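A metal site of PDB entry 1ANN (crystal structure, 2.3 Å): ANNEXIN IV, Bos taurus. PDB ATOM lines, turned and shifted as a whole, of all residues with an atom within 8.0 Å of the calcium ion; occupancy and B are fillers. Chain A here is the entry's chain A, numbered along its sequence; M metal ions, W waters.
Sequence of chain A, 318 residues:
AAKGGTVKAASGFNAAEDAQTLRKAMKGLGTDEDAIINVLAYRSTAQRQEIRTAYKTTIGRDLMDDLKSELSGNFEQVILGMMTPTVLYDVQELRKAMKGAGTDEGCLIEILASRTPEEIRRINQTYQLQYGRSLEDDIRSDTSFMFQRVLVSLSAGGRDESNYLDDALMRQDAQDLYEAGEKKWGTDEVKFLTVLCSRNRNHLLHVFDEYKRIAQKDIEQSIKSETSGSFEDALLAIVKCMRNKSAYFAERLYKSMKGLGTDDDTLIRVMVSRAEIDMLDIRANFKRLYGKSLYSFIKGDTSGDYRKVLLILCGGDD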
ATOM      1  N   TYR A 254      12.091 -15.124  -1.662  1.00  0.00           N
ATOM      2  CA  TYR A 254      11.909 -13.993  -0.769  1.00  0.00           C
ATOM      3  C   TYR A 254      12.328 -12.682  -1.479  1.00  0.00           C
ATOM      4  O   TYR A 254      11.572 -11.714  -1.508  1.00  0.00           O
ATOM      5  CB  TYR A 254      12.768 -14.192   0.477  1.00  0.00           C
ATOM      6  CG  TYR A 254      12.728 -13.019   1.425  1.00  0.00           C
ATOM      7  CD1 TYR A 254      11.605 -12.774   2.198  1.00  0.00           C
ATOM      8  CD2 TYR A 254      13.842 -12.182   1.567  1.00  0.00           C
ATOM      9  CE1 TYR A 254      11.579 -11.715   3.107  1.00  0.00           C
ATOM     10  CE2 TYR A 254      13.830 -11.121   2.480  1.00  0.00           C
ATOM     11  CZ  TYR A 254      12.699 -10.896   3.243  1.00  0.00           C
ATOM     12  OH  TYR A 254      12.691  -9.874   4.182  1.00  0.00           O
ATOM     13  N   LYS A 255      13.518 -12.658  -2.059  1.00  0.00           N
ATOM     14  CA  LYS A 255      13.991 -11.471  -2.739  1.00  0.00           C
ATOM     15  C   LYS A 255      13.196 -11.106  -3.982  1.00  0.00           C
ATOM     16  O   LYS A 255      13.249  -9.956  -4.410  1.00  0.00           O
ATOM     17  CB  LYS A 255      15.466 -11.573  -3.060  1.00  0.00           C
ATOM     18  CG  LYS A 255      16.357 -11.584  -1.834  1.00  0.00           C
ATOM     19  CD  LYS A 255      17.798 -11.802  -2.225  1.00  0.00           C
ATOM     20  CE  LYS A 255      18.714 -11.803  -1.012  1.00  0.00           C
ATOM     21  NZ  LYS A 255      20.109 -12.187  -1.393  1.00  0.00           N
ATOM     22  N   SER A 256      12.499 -12.069  -4.587  1.00  0.00           N
ATOM     23  CA  SER A 256      11.687 -11.786  -5.788  1.00  0.00           C
ATOM     24  C   SER A 256      10.363 -11.100  -5.419  1.00  0.00           C
ATOM     25  O   SER A 256       9.758 -10.438  -6.244  1.00  0.00           O
ATOM     26  CB  SER A 256      11.436 -13.051  -6.611  1.00  0.00           C
ATOM     27  OG  SER A 256      10.456 -13.905  -6.032  1.00  0.00           O
ATOM     28  N   MET A 257       9.956 -11.200  -4.154  1.00  0.00           N
ATOM     29  CA  MET A 257       8.718 -10.587  -3.719  1.00  0.00           C
ATOM     30  C   MET A 257       8.869  -9.504  -2.673  1.00  0.00           C
ATOM     31  O   MET A 257       7.954  -8.707  -2.491  1.00  0.00           O
ATOM     32  CB  MET A 257       7.792 -11.651  -3.182  1.00  0.00           C
ATOM     33  CG  MET A 257       7.347 -12.627  -4.231  1.00  0.00           C
ATOM     34  SD  MET A 257       6.264 -13.811  -3.511  1.00  0.00           S
ATOM     35  CE  MET A 257       7.458 -15.047  -2.984  1.00  0.00           C
ATOM     36  N   LYS A 258       9.963  -9.503  -1.942  1.00  0.00           N
ATOM     37  CA  LYS A 258      10.159  -8.490  -0.910  1.00  0.00           C
ATOM     38  C   LYS A 258      10.226  -7.088  -1.511  1.00  0.00           C
ATOM     39  O   LYS A 258      10.955  -6.859  -2.471  1.00  0.00           O
ATOM     40  CB  LYS A 258      11.440  -8.792  -0.125  1.00  0.00           C
ATOM     41  CG  LYS A 258      11.662  -7.929   1.100  1.00  0.00           C
ATOM     42  CD  LYS A 258      10.466  -8.007   2.056  1.00  0.00           C
ATOM     43  CE  LYS A 258      10.739  -7.284   3.390  1.00  0.00           C
ATOM     44  NZ  LYS A 258      10.987  -5.794   3.281  1.00  0.00           N
ATOM     45  N   GLY A 259       9.488  -6.147  -0.919  1.00  0.00           N
ATOM     46  CA  GLY A 259       9.501  -4.760  -1.377  1.00  0.00           C
ATOM     47  C   GLY A 259       8.434  -4.411  -2.413  1.00  0.00           C
ATOM     48  O   GLY A 259       7.561  -5.227  -2.698  1.00  0.00           O
ATOM     49  N   LEU A 260       8.458  -3.194  -2.941  1.00  0.00           N
ATOM     50  CA  LEU A 260       7.504  -2.747  -3.954  1.00  0.00           C
ATOM     51  C   LEU A 260       7.747  -3.545  -5.242  1.00  0.00           C
ATOM     52  O   LEU A 260       8.888  -3.644  -5.711  1.00  0.00           O
ATOM     53  CB  LEU A 260       7.742  -1.258  -4.278  1.00  0.00           C
ATOM     54  CG  LEU A 260       7.466  -0.200  -3.229  1.00  0.00           C
ATOM     55  CD1 LEU A 260       8.150   1.063  -3.632  1.00  0.00           C
ATOM     56  CD2 LEU A 260       5.984   0.050  -3.112  1.00  0.00           C
ATOM     57  N   GLY A 261       6.683  -4.095  -5.815  1.00  0.00           N
ATOM     58  CA  GLY A 261       6.832  -4.874  -7.036  1.00  0.00           C
ATOM     59  C   GLY A 261       7.173  -6.344  -6.847  1.00  0.00           C
ATOM     60  O   GLY A 261       7.148  -6.868  -5.740  1.00  0.00           O
ATOM     61  N   THR A 262       7.510  -7.018  -7.935  1.00  0.00           N
ATOM     62  CA  THR A 262       7.827  -8.437  -7.898  1.00  0.00           C
ATOM     63  C   THR A 262       8.785  -8.719  -9.037  1.00  0.00           C
ATOM     64  O   THR A 262       8.835  -7.973 -10.005  1.00  0.00           O
ATOM     65  CB  THR A 262       6.541  -9.262  -8.185  1.00  0.00           C
ATOM     66  OG1 THR A 262       5.443  -8.709  -7.444  1.00  0.00           O
ATOM     67  CG2 THR A 262       6.725 -10.773  -7.892  1.00  0.00           C
ATOM     68  N   ASP A 263       9.600  -9.759  -8.902  1.00  0.00           N
ATOM     69  CA  ASP A 263      10.478 -10.146  -9.978  1.00  0.00           C
ATOM     70  C   ASP A 263       9.778 -11.431 -10.450  1.00  0.00           C
ATOM     71  O   ASP A 263      10.136 -12.529 -10.058  1.00  0.00           O
ATOM     72  CB  ASP A 263      11.896 -10.391  -9.469  1.00  0.00           C
ATOM     73  CG  ASP A 263      12.534  -9.121  -8.896  1.00  0.00           C
ATOM     74  OD1 ASP A 263      12.513  -8.079  -9.590  1.00  0.00           O
ATOM     75  OD2 ASP A 263      13.006  -9.130  -7.748  1.00  0.00           O
ATOM     76  N   PHE A 297       3.118 -14.721   1.199  1.00  0.00           N
ATOM     77  CA  PHE A 297       3.946 -13.799   0.416  1.00  0.00           C
ATOM     78  C   PHE A 297       3.438 -13.753  -1.018  1.00  0.00           C
ATOM     79  O   PHE A 297       3.205 -12.686  -1.590  1.00  0.00           O
ATOM     80  CB  PHE A 297       5.409 -14.223   0.430  1.00  0.00           C
ATOM     81  CG  PHE A 297       6.309 -13.293   1.205  1.00  0.00           C
ATOM     82  CD1 PHE A 297       6.315 -13.302   2.589  1.00  0.00           C
ATOM     83  CD2 PHE A 297       7.178 -12.451   0.536  1.00  0.00           C
ATOM     84  CE1 PHE A 297       7.184 -12.498   3.291  1.00  0.00           C
ATOM     85  CE2 PHE A 297       8.039 -11.636   1.232  1.00  0.00           C
ATOM     86  CZ  PHE A 297       8.039 -11.658   2.618  1.00  0.00           C
ATOM     87  N   GLY A 300       0.175 -12.163  -1.279  1.00  0.00           N
ATOM     88  CA  GLY A 300       0.236 -10.716  -1.199  1.00  0.00           C
ATOM     89  C   GLY A 300       0.894 -10.028  -2.378  1.00  0.00           C
ATOM     90  O   GLY A 300       0.694  -8.838  -2.588  1.00  0.00           O
ATOM     91  N   ASP A 301       1.679 -10.758  -3.158  1.00  0.00           N
ATOM     92  CA  ASP A 301       2.362 -10.155  -4.285  1.00  0.00           C
ATOM     93  C   ASP A 301       1.765 -10.382  -5.644  1.00  0.00           C
ATOM     94  O   ASP A 301       2.252  -9.812  -6.620  1.00  0.00           O
ATOM     95  CB  ASP A 301       3.805 -10.639  -4.339  1.00  0.00           C
ATOM     96  CG  ASP A 301       4.772  -9.541  -4.013  1.00  0.00           C
ATOM     97  OD1 ASP A 301       4.593  -8.884  -2.981  1.00  0.00           O
ATOM     98  OD2 ASP A 301       5.705  -9.328  -4.788  1.00  0.00           O
ATOM     99  N   THR A 302       0.718 -11.198  -5.728  1.00  0.00           N
ATOM    100  CA  THR A 302       0.118 -11.526  -7.010  1.00  0.00           C
ATOM    101  C   THR A 302      -1.408 -11.444  -6.977  1.00  0.00           C
ATOM    102  O   THR A 302      -2.005 -11.161  -5.924  1.00  0.00           O
ATOM    103  CB  THR A 302       0.619 -12.926  -7.501  1.00  0.00           C
ATOM    104  OG1 THR A 302       0.226 -13.936  -6.559  1.00  0.00           O
ATOM    105  CG2 THR A 302       2.141 -12.957  -7.593  1.00  0.00           C
HETATM  106 CA    CA M   1       6.395  -7.182  -3.519  1.00  0.00          CA
HETATM  107  O   HOH W   1       5.611  -6.488  -1.170  1.00  0.00           O
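The side-chain hydroxyl (OG1) of Thr 262 lies within hydrogen-bond range of the backbone carbonyl oxygen (O) of Asp 301.
The calcium ion is bound by the backbone carbonyl oxygen (O) of Gly 261 (2.4 Å), the backbone carbonyl oxygen (O) of Met 257 (2.4 Å), the backbone carbonyl oxygen (O) of Gly 259 (2.4 Å), the side-chain carboxylate (OD1) of Asp 301 (2.5 Å), water W1 (2.6 Å) and the side-chain carboxylate (OD2) of Asp 301 (2.6 Å).
Of the 14 residues printed, 4 come within 4 Å of the calcium ion. The nearest printed residue that does not touch the calcium ion is Leu 260 (4.2 Å).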
